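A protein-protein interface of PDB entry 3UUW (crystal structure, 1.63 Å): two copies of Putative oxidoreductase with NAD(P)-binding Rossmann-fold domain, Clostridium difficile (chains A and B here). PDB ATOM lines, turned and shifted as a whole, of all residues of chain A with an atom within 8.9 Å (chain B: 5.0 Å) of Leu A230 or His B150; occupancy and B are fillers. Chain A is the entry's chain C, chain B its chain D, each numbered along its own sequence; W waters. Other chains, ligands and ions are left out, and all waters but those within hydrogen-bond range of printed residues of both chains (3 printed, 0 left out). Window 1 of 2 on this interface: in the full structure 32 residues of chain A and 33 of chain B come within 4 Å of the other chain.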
ATOM      1  N   ILE A 135      -7.107  14.670 -10.407  1.00  0.00           N
ATOM      2  CA  ILE A 135      -6.376  14.484  -9.142  1.00  0.00           C
ATOM      3  C   ILE A 135      -5.865  15.807  -8.572  1.00  0.00           C
ATOM      4  O   ILE A 135      -5.913  16.023  -7.346  1.00  0.00           O
ATOM      5  CB  ILE A 135      -5.279  13.397  -9.190  1.00  0.00           C
ATOM      6  CG1 ILE A 135      -4.128  13.751 -10.128  1.00  0.00           C
ATOM      7  CG2 ILE A 135      -5.932  12.058  -9.578  1.00  0.00           C
ATOM      8  CD1 ILE A 135      -2.928  12.809  -9.984  1.00  0.00           C
ATOM      9  N   ALA A 139      -7.083  17.109  -4.737  1.00  0.00           N
ATOM     10  CA  ALA A 139      -6.081  17.020  -3.694  1.00  0.00           C
ATOM     11  C   ALA A 139      -6.154  18.244  -2.788  1.00  0.00           C
ATOM     12  O   ALA A 139      -6.223  19.373  -3.273  1.00  0.00           O
ATOM     13  CB  ALA A 139      -4.697  16.915  -4.304  1.00  0.00           C
ATOM     14  N   THR A 140      -6.159  18.015  -1.483  1.00  0.00           N
ATOM     15  CA  THR A 140      -6.025  19.117  -0.521  1.00  0.00           C
ATOM     16  C   THR A 140      -5.051  18.654   0.549  1.00  0.00           C
ATOM     17  O   THR A 140      -4.977  17.471   0.843  1.00  0.00           O
ATOM     18  CB  THR A 140      -7.360  19.557   0.129  1.00  0.00           C
ATOM     19  OG1 THR A 140      -7.948  18.460   0.835  1.00  0.00           O
ATOM     20  CG2 THR A 140      -8.340  20.074  -0.919  1.00  0.00           C
ATOM     21  N   GLU A 141      -4.315  19.598   1.125  1.00  0.00           N
ATOM     22  CA  GLU A 141      -3.322  19.311   2.157  1.00  0.00           C
ATOM     23  C   GLU A 141      -2.332  18.234   1.701  1.00  0.00           C
ATOM     24  O   GLU A 141      -2.134  17.225   2.365  1.00  0.00           O
ATOM     25  CB  GLU A 141      -3.991  18.930   3.472  1.00  0.00           C
ATOM     26  CG  GLU A 141      -4.968  20.006   3.988  1.00  0.00           C
ATOM     27  CD  GLU A 141      -5.586  19.659   5.333  1.00  0.00           C
ATOM     28  OE1 GLU A 141      -4.837  19.583   6.324  1.00  0.00           O
ATOM     29  OE2 GLU A 141      -6.822  19.479   5.410  1.00  0.00           O
ATOM     30  N   ILE A 142      -1.738  18.503   0.552  1.00  0.00           N
ATOM     31  CA  ILE A 142      -0.726  17.651  -0.057  1.00  0.00           C
ATOM     32  C   ILE A 142       0.544  17.608   0.818  1.00  0.00           C
ATOM     33  O   ILE A 142       0.983  18.653   1.340  1.00  0.00           O
ATOM     34  CB  ILE A 142      -0.376  18.190  -1.463  1.00  0.00           C
ATOM     35  CG1 ILE A 142      -1.589  18.102  -2.402  1.00  0.00           C
ATOM     36  CG2 ILE A 142       0.795  17.431  -2.084  1.00  0.00           C
ATOM     37  CD1 ILE A 142      -1.294  18.649  -3.807  1.00  0.00           C
ATOM     38  N   VAL A 143       1.118  16.415   1.008  1.00  0.00           N
ATOM     39  CA  VAL A 143       2.385  16.294   1.723  1.00  0.00           C
ATOM     40  C   VAL A 143       3.525  15.904   0.811  1.00  0.00           C
ATOM     41  O   VAL A 143       4.681  16.099   1.159  1.00  0.00           O
ATOM     42  CB  VAL A 143       2.333  15.323   2.928  1.00  0.00           C
ATOM     43  CG1 VAL A 143       1.332  15.831   3.963  1.00  0.00           C
ATOM     44  CG2 VAL A 143       2.006  13.865   2.491  1.00  0.00           C
ATOM     45  N   SER A 144       3.215  15.340  -0.355  1.00  0.00           N
ATOM     46  CA  SER A 144       4.287  14.927  -1.270  1.00  0.00           C
ATOM     47  C   SER A 144       3.716  14.576  -2.628  1.00  0.00           C
ATOM     48  O   SER A 144       2.573  14.134  -2.709  1.00  0.00           O
ATOM     49  CB  SER A 144       4.985  13.704  -0.665  1.00  0.00           C
ATOM     50  OG  SER A 144       6.143  13.308  -1.393  1.00  0.00           O
ATOM     51  N   ILE A 145       4.509  14.761  -3.691  1.00  0.00           N
ATOM     52  CA  ILE A 145       4.102  14.331  -4.999  1.00  0.00           C
ATOM     53  C   ILE A 145       5.295  13.609  -5.631  1.00  0.00           C
ATOM     54  O   ILE A 145       6.435  14.057  -5.483  1.00  0.00           O
ATOM     55  CB  ILE A 145       3.668  15.501  -5.899  1.00  0.00           C
ATOM     56  CG1 ILE A 145       2.486  16.248  -5.297  1.00  0.00           C
ATOM     57  CG2 ILE A 145       3.314  14.978  -7.318  1.00  0.00           C
ATOM     58  CD1 ILE A 145       1.950  17.374  -6.173  1.00  0.00           C
ATOM     59  N   ASN A 146       5.014  12.479  -6.285  1.00  0.00           N
ATOM     60  CA  ASN A 146       6.026  11.740  -7.046  1.00  0.00           C
ATOM     61  C   ASN A 146       5.626  11.678  -8.514  1.00  0.00           C
ATOM     62  O   ASN A 146       4.490  11.338  -8.823  1.00  0.00           O
ATOM     63  CB  ASN A 146       6.166  10.330  -6.473  1.00  0.00           C
ATOM     64  CG  ASN A 146       6.575  10.337  -5.010  1.00  0.00           C
ATOM     65  OD1 ASN A 146       7.487  11.067  -4.605  1.00  0.00           O
ATOM     66  ND2 ASN A 146       5.898   9.520  -4.205  1.00  0.00           N
ATOM     67  N   ASN A 209       5.286  23.997   1.267  1.00  0.00           N
ATOM     68  CA  ASN A 209       4.304  23.068   1.826  1.00  0.00           C
ATOM     69  C   ASN A 209       4.580  21.589   1.564  1.00  0.00           C
ATOM     70  O   ASN A 209       4.172  20.713   2.335  1.00  0.00           O
ATOM     71  CB  ASN A 209       2.927  23.447   1.280  1.00  0.00           C
ATOM     72  CG  ASN A 209       2.463  24.801   1.785  1.00  0.00           C
ATOM     73  OD1 ASN A 209       2.300  24.996   2.988  1.00  0.00           O
ATOM     74  ND2 ASN A 209       2.231  25.735   0.865  1.00  0.00           N
ATOM     75  N   PHE A 210       5.265  21.300   0.471  1.00  0.00           N
ATOM     76  CA  PHE A 210       5.587  19.925   0.159  1.00  0.00           C
ATOM     77  C   PHE A 210       6.654  19.909  -0.926  1.00  0.00           C
ATOM     78  O   PHE A 210       6.972  20.953  -1.502  1.00  0.00           O
ATOM     79  CB  PHE A 210       4.338  19.132  -0.288  1.00  0.00           C
ATOM     80  CG  PHE A 210       3.608  19.731  -1.478  1.00  0.00           C
ATOM     81  CD1 PHE A 210       3.993  19.426  -2.769  1.00  0.00           C
ATOM     82  CD2 PHE A 210       2.529  20.585  -1.293  1.00  0.00           C
ATOM     83  CE1 PHE A 210       3.317  19.960  -3.862  1.00  0.00           C
ATOM     84  CE2 PHE A 210       1.848  21.120  -2.383  1.00  0.00           C
ATOM     85  CZ  PHE A 210       2.258  20.819  -3.664  1.00  0.00           C
ATOM     86  N   SER A 211       7.200  18.728  -1.170  1.00  0.00           N
ATOM     87  CA  SER A 211       8.197  18.527  -2.229  1.00  0.00           C
ATOM     88  C   SER A 211       7.648  17.623  -3.325  1.00  0.00           C
ATOM     89  O   SER A 211       6.718  16.821  -3.112  1.00  0.00           O
ATOM     90  CB  SER A 211       9.464  17.895  -1.661  1.00  0.00           C
ATOM     91  OG  SER A 211      10.045  18.715  -0.678  1.00  0.00           O
ATOM     92  N   ASN A 213       9.072  14.837  -6.104  1.00  0.00           N
ATOM     93  CA  ASN A 213      10.158  13.986  -6.530  1.00  0.00           C
ATOM     94  C   ASN A 213       9.963  13.554  -7.977  1.00  0.00           C
ATOM     95  O   ASN A 213       9.013  12.835  -8.303  1.00  0.00           O
ATOM     96  CB  ASN A 213      10.195  12.766  -5.615  1.00  0.00           C
ATOM     97  CG  ASN A 213      10.389  13.160  -4.158  1.00  0.00           C
ATOM     98  OD1 ASN A 213      11.480  13.557  -3.769  1.00  0.00           O
ATOM     99  ND2 ASN A 213       9.308  13.122  -3.366  1.00  0.00           N
ATOM    100  N   VAL A 227       1.888   9.791 -11.942  1.00  0.00           N
ATOM    101  CA  VAL A 227       1.851  10.901 -11.006  1.00  0.00           C
ATOM    102  C   VAL A 227       1.155  10.344  -9.757  1.00  0.00           C
ATOM    103  O   VAL A 227       0.097   9.718  -9.857  1.00  0.00           O
ATOM    104  CB  VAL A 227       1.052  12.122 -11.512  1.00  0.00           C
ATOM    105  CG1 VAL A 227       0.878  13.180 -10.416  1.00  0.00           C
ATOM    106  CG2 VAL A 227       1.722  12.734 -12.722  1.00  0.00           C
ATOM    107  N   GLU A 228       1.796  10.503  -8.615  1.00  0.00           N
ATOM    108  CA  GLU A 228       1.223  10.109  -7.327  1.00  0.00           C
ATOM    109  C   GLU A 228       1.223  11.287  -6.385  1.00  0.00           C
ATOM    110  O   GLU A 228       2.277  11.899  -6.177  1.00  0.00           O
ATOM    111  CB  GLU A 228       2.063   8.998  -6.732  1.00  0.00           C
ATOM    112  CG  GLU A 228       1.649   8.482  -5.382  1.00  0.00           C
ATOM    113  CD  GLU A 228       2.565   7.355  -4.976  1.00  0.00           C
ATOM    114  OE1 GLU A 228       3.739   7.652  -4.643  1.00  0.00           O
ATOM    115  OE2 GLU A 228       2.131   6.179  -5.035  1.00  0.00           O
ATOM    116  N   ILE A 229       0.065  11.580  -5.796  1.00  0.00           N
ATOM    117  CA  ILE A 229      -0.094  12.665  -4.848  1.00  0.00           C
ATOM    118  C   ILE A 229      -0.487  12.089  -3.494  1.00  0.00           C
ATOM    119  O   ILE A 229      -1.483  11.373  -3.375  1.00  0.00           O
ATOM    120  CB  ILE A 229      -1.156  13.673  -5.271  1.00  0.00           C
ATOM    121  CG1 ILE A 229      -0.828  14.272  -6.647  1.00  0.00           C
ATOM    122  CG2 ILE A 229      -1.289  14.806  -4.222  1.00  0.00           C
ATOM    123  CD1 ILE A 229      -1.971  15.166  -7.168  1.00  0.00           C
ATOM    124  N   LEU A 230       0.349  12.350  -2.501  1.00  0.00           N
ATOM    125  CA  LEU A 230       0.068  11.972  -1.120  1.00  0.00           C
ATOM    126  C   LEU A 230      -0.534  13.197  -0.472  1.00  0.00           C
ATOM    127  O   LEU A 230       0.051  14.283  -0.548  1.00  0.00           O
ATOM    128  CB  LEU A 230       1.360  11.620  -0.375  1.00  0.00           C
ATOM    129  CG  LEU A 230       2.185  10.446  -0.886  1.00  0.00           C
ATOM    130  CD1 LEU A 230       3.370  10.241   0.052  1.00  0.00           C
ATOM    131  CD2 LEU A 230       1.366   9.188  -0.969  1.00  0.00           C
ATOM    132  N   SER A 231      -1.690  13.039   0.164  1.00  0.00           N
ATOM    133  CA  SER A 231      -2.334  14.131   0.865  1.00  0.00           C
ATOM    134  C   SER A 231      -3.010  13.586   2.104  1.00  0.00           C
ATOM    135  O   SER A 231      -3.046  12.383   2.340  1.00  0.00           O
ATOM    136  CB  SER A 231      -3.306  14.887  -0.048  1.00  0.00           C
ATOM    137  OG  SER A 231      -4.347  14.054  -0.502  1.00  0.00           O
ATOM    138  N   LYS A 232      -3.555  14.488   2.908  1.00  0.00           N
ATOM    139  CA  LYS A 232      -4.251  14.088   4.111  1.00  0.00           C
ATOM    140  C   LYS A 232      -5.336  13.055   3.810  1.00  0.00           C
ATOM    141  O   LYS A 232      -6.262  13.318   3.030  1.00  0.00           O
ATOM    142  CB  LYS A 232      -4.885  15.299   4.778  1.00  0.00           C
ATOM    143  CG  LYS A 232      -5.984  14.924   5.766  1.00  0.00           C
ATOM    144  CD  LYS A 232      -6.497  16.106   6.559  1.00  0.00           C
ATOM    145  CE  LYS A 232      -5.473  16.593   7.578  1.00  0.00           C
ATOM    146  NZ  LYS A 232      -6.047  17.608   8.525  1.00  0.00           N
ATOM    147  N   GLY A 233      -5.193  11.870   4.397  1.00  0.00           N
ATOM    148  CA  GLY A 233      -6.179  10.813   4.254  1.00  0.00           C
ATOM    149  C   GLY A 233      -6.321  10.181   2.885  1.00  0.00           C
ATOM    150  O   GLY A 233      -7.283   9.470   2.660  1.00  0.00           O
ATOM    151  N   LYS A 234      -5.355  10.372   1.980  1.00  0.00           N
ATOM    152  CA  LYS A 234      -5.555   9.930   0.621  1.00  0.00           C
ATOM    153  C   LYS A 234      -4.273   9.784  -0.172  1.00  0.00           C
ATOM    154  O   LYS A 234      -3.310  10.540   0.027  1.00  0.00           O
ATOM    155  CB  LYS A 234      -6.420  10.988  -0.077  1.00  0.00           C
ATOM    156  CG  LYS A 234      -7.034  10.599  -1.398  1.00  0.00           C
ATOM    157  CD  LYS A 234      -7.652  11.812  -2.112  1.00  0.00           C
ATOM    158  CE  LYS A 234      -8.785  12.448  -1.394  1.00  0.00           C
ATOM    159  NZ  LYS A 234      -9.303  13.630  -2.173  1.00  0.00           N
ATOM    160  N   ILE A 235      -4.257   8.793  -1.042  1.00  0.00           N
ATOM    161  CA  ILE A 235      -3.232   8.696  -2.077  1.00  0.00           C
ATOM    162  C   ILE A 235      -3.978   8.667  -3.397  1.00  0.00           C
ATOM    163  O   ILE A 235      -4.946   7.930  -3.544  1.00  0.00           O
ATOM    164  CB  ILE A 235      -2.380   7.409  -2.009  1.00  0.00           C
ATOM    165  CG1 ILE A 235      -1.700   7.246  -0.654  1.00  0.00           C
ATOM    166  CG2 ILE A 235      -1.312   7.441  -3.118  1.00  0.00           C
ATOM    167  CD1 ILE A 235      -0.907   5.911  -0.502  1.00  0.00           C
ATOM    168  N   GLN A 236      -3.532   9.475  -4.358  1.00  0.00           N
ATOM    169  CA  GLN A 236      -4.099   9.483  -5.707  1.00  0.00           C
ATOM    170  C   GLN A 236      -2.971   9.182  -6.678  1.00  0.00           C
ATOM    171  O   GLN A 236      -1.866   9.729  -6.538  1.00  0.00           O
ATOM    172  CB  GLN A 236      -4.682  10.854  -6.088  1.00  0.00           C
ATOM    173  CG  GLN A 236      -5.851  11.398  -5.255  1.00  0.00           C
ATOM    174  CD  GLN A 236      -5.904  12.930  -5.320  1.00  0.00           C
ATOM    175  OE1 GLN A 236      -5.037  13.605  -4.772  1.00  0.00           O
ATOM    176  NE2 GLN A 236      -6.913  13.463  -5.959  1.00  0.00           N
ATOM    177  N   ARG A 237      -3.235   8.309  -7.650  1.00  0.00           N
ATOM    178  CA  ARG A 237      -2.241   8.017  -8.677  1.00  0.00           C
ATOM    179  C   ARG A 237      -2.888   7.977 -10.034  1.00  0.00           C
ATOM    180  O   ARG A 237      -4.007   7.496 -10.162  1.00  0.00           O
ATOM    181  CB  ARG A 237      -1.615   6.656  -8.465  1.00  0.00           C
ATOM    182  CG  ARG A 237      -1.047   6.384  -7.187  1.00  0.00           C
ATOM    183  CD  ARG A 237      -0.342   5.011  -7.259  1.00  0.00           C
ATOM    184  NE  ARG A 237      -0.003   4.689  -5.920  1.00  0.00           N
ATOM    185  CZ  ARG A 237      -0.787   4.025  -5.100  1.00  0.00           C
ATOM    186  NH1 ARG A 237      -1.927   3.503  -5.549  1.00  0.00           N
ATOM    187  NH2 ARG A 237      -0.387   3.810  -3.858  1.00  0.00           N
ATOM    188  N   GLU A 247      -6.502   5.696  -3.008  1.00  0.00           N
ATOM    189  CA  GLU A 247      -6.437   4.905  -1.790  1.00  0.00           C
ATOM    190  C   GLU A 247      -6.945   5.797  -0.663  1.00  0.00           C
ATOM    191  O   GLU A 247      -6.363   6.846  -0.379  1.00  0.00           O
ATOM    192  CB  GLU A 247      -5.034   4.358  -1.510  1.00  0.00           C
ATOM    193  CG  GLU A 247      -4.473   3.611  -2.712  1.00  0.00           C
ATOM    194  CD  GLU A 247      -3.491   2.472  -2.416  1.00  0.00           C
ATOM    195  OE1 GLU A 247      -3.736   1.667  -1.500  1.00  0.00           O
ATOM    196  OE2 GLU A 247      -2.488   2.334  -3.170  1.00  0.00           O
ATOM    197  N   CYS B 148       8.764   3.276   0.925  1.00  0.00           N
ATOM    198  CA  CYS B 148       7.775   4.000   1.704  1.00  0.00           C
ATOM    199  C   CYS B 148       7.022   3.115   2.662  1.00  0.00           C
ATOM    200  O   CYS B 148       6.815   1.932   2.423  1.00  0.00           O
ATOM    201  CB  CYS B 148       6.776   4.717   0.822  1.00  0.00           C
ATOM    202  SG  CYS B 148       5.741   3.618  -0.146  1.00  0.00           S
ATOM    203  N   LYS B 149       6.545   3.731   3.736  1.00  0.00           N
ATOM    204  CA  LYS B 149       5.776   3.034   4.754  1.00  0.00           C
ATOM    205  C   LYS B 149       4.746   4.019   5.272  1.00  0.00           C
ATOM    206  O   LYS B 149       5.075   4.925   6.031  1.00  0.00           O
ATOM    207  CB  LYS B 149       6.660   2.507   5.885  1.00  0.00           C
ATOM    208  CG  LYS B 149       5.916   1.641   6.892  1.00  0.00           C
ATOM    209  CD  LYS B 149       6.843   1.010   7.925  1.00  0.00           C
ATOM    210  CE  LYS B 149       6.107   0.002   8.817  1.00  0.00           C
ATOM    211  NZ  LYS B 149       5.025   0.625   9.647  1.00  0.00           N
ATOM    212  N   HIS B 150       3.508   3.851   4.826  1.00  0.00           N
ATOM    213  CA  HIS B 150       2.420   4.757   5.156  1.00  0.00           C
ATOM    214  C   HIS B 150       1.363   4.099   6.021  1.00  0.00           C
ATOM    215  O   HIS B 150       1.144   2.882   5.971  1.00  0.00           O
ATOM    216  CB  HIS B 150       1.765   5.284   3.876  1.00  0.00           C
ATOM    217  CG  HIS B 150       2.729   5.916   2.918  1.00  0.00           C
ATOM    218  ND1 HIS B 150       3.727   6.772   3.326  1.00  0.00           N
ATOM    219  CD2 HIS B 150       2.819   5.853   1.565  1.00  0.00           C
ATOM    220  CE1 HIS B 150       4.389   7.210   2.270  1.00  0.00           C
ATOM    221  NE2 HIS B 150       3.865   6.660   1.191  1.00  0.00           N
ATOM    222  N   GLY B 151       0.703   4.912   6.822  1.00  0.00           N
ATOM    223  CA  GLY B 151      -0.328   4.397   7.695  1.00  0.00           C
ATOM    224  C   GLY B 151      -1.643   5.106   7.563  1.00  0.00           C
ATOM    225  O   GLY B 151      -1.705   6.272   7.123  1.00  0.00           O
ATOM    226  N   LEU B 152      -2.699   4.369   7.911  1.00  0.00           N
ATOM    227  CA  LEU B 152      -4.041   4.867   7.924  1.00  0.00           C
ATOM    228  C   LEU B 152      -4.364   5.168   9.389  1.00  0.00           C
ATOM    229  O   LEU B 152      -4.263   4.279  10.240  1.00  0.00           O
ATOM    230  CB  LEU B 152      -5.011   3.813   7.385  1.00  0.00           C
ATOM    231  CG  LEU B 152      -6.480   4.200   7.504  1.00  0.00           C
ATOM    232  CD1 LEU B 152      -6.795   5.415   6.612  1.00  0.00           C
ATOM    233  CD2 LEU B 152      -7.456   3.041   7.227  1.00  0.00           C
ATOM    234  N   PHE B 200       4.596  13.660   8.453  1.00  0.00           N
ATOM    235  CA  PHE B 200       5.297  13.134   7.282  1.00  0.00           C
ATOM    236  C   PHE B 200       6.799  13.335   7.383  1.00  0.00           C
ATOM    237  O   PHE B 200       7.261  14.377   7.844  1.00  0.00           O
ATOM    238  CB  PHE B 200       4.761  13.840   6.019  1.00  0.00           C
ATOM    239  CG  PHE B 200       5.450  13.411   4.729  1.00  0.00           C
ATOM    240  CD1 PHE B 200       6.472  14.159   4.192  1.00  0.00           C
ATOM    241  CD2 PHE B 200       5.061  12.254   4.068  1.00  0.00           C
ATOM    242  CE1 PHE B 200       7.108  13.751   3.011  1.00  0.00           C
ATOM    243  CE2 PHE B 200       5.688  11.847   2.914  1.00  0.00           C
ATOM    244  CZ  PHE B 200       6.704  12.592   2.374  1.00  0.00           C
ATOM    245  N   SER B 215      10.304   7.497   2.590  1.00  0.00           N
ATOM    246  CA  SER B 215       9.182   8.307   3.038  1.00  0.00           C
ATOM    247  C   SER B 215       8.214   7.546   3.939  1.00  0.00           C
ATOM    248  O   SER B 215       8.056   6.315   3.870  1.00  0.00           O
ATOM    249  CB  SER B 215       8.414   8.847   1.864  1.00  0.00           C
ATOM    250  OG  SER B 215       7.845   7.782   1.137  1.00  0.00           O
ATOM    251  N   MET B 216       7.506   8.322   4.741  1.00  0.00           N
ATOM    252  CA  MET B 216       6.541   7.777   5.641  1.00  0.00           C
ATOM    253  C   MET B 216       5.499   8.856   5.948  1.00  0.00           C
ATOM    254  O   MET B 216       5.837   9.913   6.476  1.00  0.00           O
ATOM    255  CB  MET B 216       7.242   7.305   6.933  1.00  0.00           C
ATOM    256  CG  MET B 216       6.305   7.130   8.122  1.00  0.00           C
ATOM    257  SD  MET B 216       7.137   6.434   9.572  1.00  0.00           S
ATOM    258  CE  MET B 216       7.213   4.706   9.109  1.00  0.00           C
ATOM    259  N   HIS B 217       4.253   8.570   5.568  1.00  0.00           N
ATOM    260  CA  HIS B 217       3.103   9.420   5.862  1.00  0.00           C
ATOM    261  C   HIS B 217       2.212   8.705   6.863  1.00  0.00           C
ATOM    262  O   HIS B 217       1.697   7.595   6.600  1.00  0.00           O
ATOM    263  CB  HIS B 217       2.335   9.751   4.597  1.00  0.00           C
ATOM    264  CG  HIS B 217       1.303  10.804   4.780  1.00  0.00           C
ATOM    265  ND1 HIS B 217       0.201  10.904   3.963  1.00  0.00           N
ATOM    266  CD2 HIS B 217       1.194  11.804   5.687  1.00  0.00           C
ATOM    267  CE1 HIS B 217      -0.532  11.931   4.343  1.00  0.00           C
ATOM    268  NE2 HIS B 217       0.034  12.482   5.407  1.00  0.00           N
ATOM    269  N   SER B 220      -2.168   8.848   5.951  1.00  0.00           N
ATOM    270  CA  SER B 220      -2.409   8.484   4.573  1.00  0.00           C
ATOM    271  C   SER B 220      -3.814   7.858   4.388  1.00  0.00           C
ATOM    272  O   SER B 220      -4.679   7.918   5.294  1.00  0.00           O
ATOM    273  CB  SER B 220      -1.300   7.512   4.145  1.00  0.00           C
ATOM    274  OG  SER B 220      -1.277   7.340   2.744  1.00  0.00           O
ATOM    275  N   THR B 222      -4.250   4.601   3.361  1.00  0.00           N
ATOM    276  CA  THR B 222      -4.203   3.166   3.570  1.00  0.00           C
ATOM    277  C   THR B 222      -2.913   2.831   4.304  1.00  0.00           C
ATOM    278  O   THR B 222      -2.009   3.677   4.402  1.00  0.00           O
ATOM    279  CB  THR B 222      -4.257   2.401   2.227  1.00  0.00           C
ATOM    280  OG1 THR B 222      -4.637   1.036   2.444  1.00  0.00           O
ATOM    281  CG2 THR B 222      -2.933   2.499   1.481  1.00  0.00           C
ATOM    282  N   LYS B 223      -2.850   1.621   4.844  1.00  0.00           N
ATOM    283  CA  LYS B 223      -1.615   1.105   5.394  1.00  0.00           C
ATOM    284  C   LYS B 223      -0.910   0.388   4.256  1.00  0.00           C
ATOM    285  O   LYS B 223      -1.451  -0.572   3.697  1.00  0.00           O
ATOM    286  CB  LYS B 223      -1.875   0.132   6.520  1.00  0.00           C
ATOM    287  CG  LYS B 223      -0.623  -0.349   7.223  1.00  0.00           C
ATOM    288  CD  LYS B 223      -0.985  -1.379   8.286  1.00  0.00           C
ATOM    289  CE  LYS B 223       0.231  -2.156   8.787  1.00  0.00           C
ATOM    290  NZ  LYS B 223       1.242  -1.275   9.420  1.00  0.00           N
ATOM    291  N   LEU B 224       0.252   0.871   3.880  1.00  0.00           N
ATOM    292  CA  LEU B 224       1.022   0.162   2.870  1.00  0.00           C
ATOM    293  C   LEU B 224       2.521   0.315   3.083  1.00  0.00           C
ATOM    294  O   LEU B 224       2.976   1.259   3.713  1.00  0.00           O
ATOM    295  CB  LEU B 224       0.612   0.615   1.472  1.00  0.00           C
ATOM    296  CG  LEU B 224       1.036   1.941   0.876  1.00  0.00           C
ATOM    297  CD1 LEU B 224       2.534   1.963   0.572  1.00  0.00           C
ATOM    298  CD2 LEU B 224       0.263   2.167  -0.425  1.00  0.00           C
HETATM  299  O   HOH W   1       4.690   6.779  -1.587  1.00  0.00           O
HETATM  300  O   HOH W   2      -0.865   9.783   1.648  1.00  0.00           O
HETATM  301  O   HOH W   3      -5.745   0.578  -0.009  1.00  0.00           O
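The backbone carbonyl oxygen (O) of Leu A230 lies within hydrogen-bond range of the backbone NH (N) of Val A143 (2.8 Å). O of Ser A144 is in hydrogen-bond range of N of Leu A230, 2.9 Å away. The guanidinium group of Arg A237 is in salt-bridge range of the side-chain carboxylate of Glu A247. The backbone NH (N) of His B217 is in hydrogen-bond range of a ring nitrogen (ND1) of His B150, at 2.9 Å. N of His B150 lies within hydrogen-bond range of O of Leu B224, at 2.9 Å. The backbone carbonyl oxygen of His B217 is in hydrogen-bond range of the backbone NH of Gly B151 (2.9 Å).
CG2 of Val A143 touches CD2 of Phe B200, 3.8 Å away. Val A143 touches His B217 (CG2 to CE1, 3.7 Å). CZ of Phe B200 touches CB of Ser A144, at 3.7 Å. CD1 of Leu A230 touches NE2 of His B150, at 3.8 Å. Ser A231 touches His B217. O of Ser B220 touches CA of Gly A233 (3.4 Å). Lys A234 touches Ser B220. NH2 of Arg A237 touches CD2 of Leu B224, 3.9 Å away. Glu A247 touches Thr B222. Glu A247 touches Leu B224.
Of the printed residues of chain B, Leu A230 touches His B150. Printed residues of chain A within 4 Å of His B150: Leu A230 (3.8 Å). Of the printed residues of chain B, Gly A233 touches Ser B220 (3.4 Å). Of the printed residues of chain A, Thr B222 touches Glu A247. Of the printed residues of chain B, Lys A234 touches Ser B220. Ile A142 touches none of the printed residues of chain B. The nearest printed residue of chain A that does not touch His B150 is Ile A235 (4.3 Å). The nearest printed residue of chain A that does not touch Leu B224 is Glu A228 (6.4 Å).
No position is printed for both chains. Of the 12 pairs that touch across the chains among the printed residues, none has its exchanged pair printed and touching as well.
Water W2 lies within hydrogen-bond range of OG of Ser B220, ND1 of His B217, O of Lys A234 and O of Ser A231. Water W3 bridges OE1 of Glu A247 (2.7 Å) and OG1 of Thr B222 (2.7 Å). Water W1 lies within hydrogen-bond range of a ring nitrogen (NE2) of His B150 (2.9 Å), the side-chain carboxylate (OE1) of Glu A228 (3.3 Å) and the side-chain sulfur (SG) of Cys B148 (3.6 Å).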
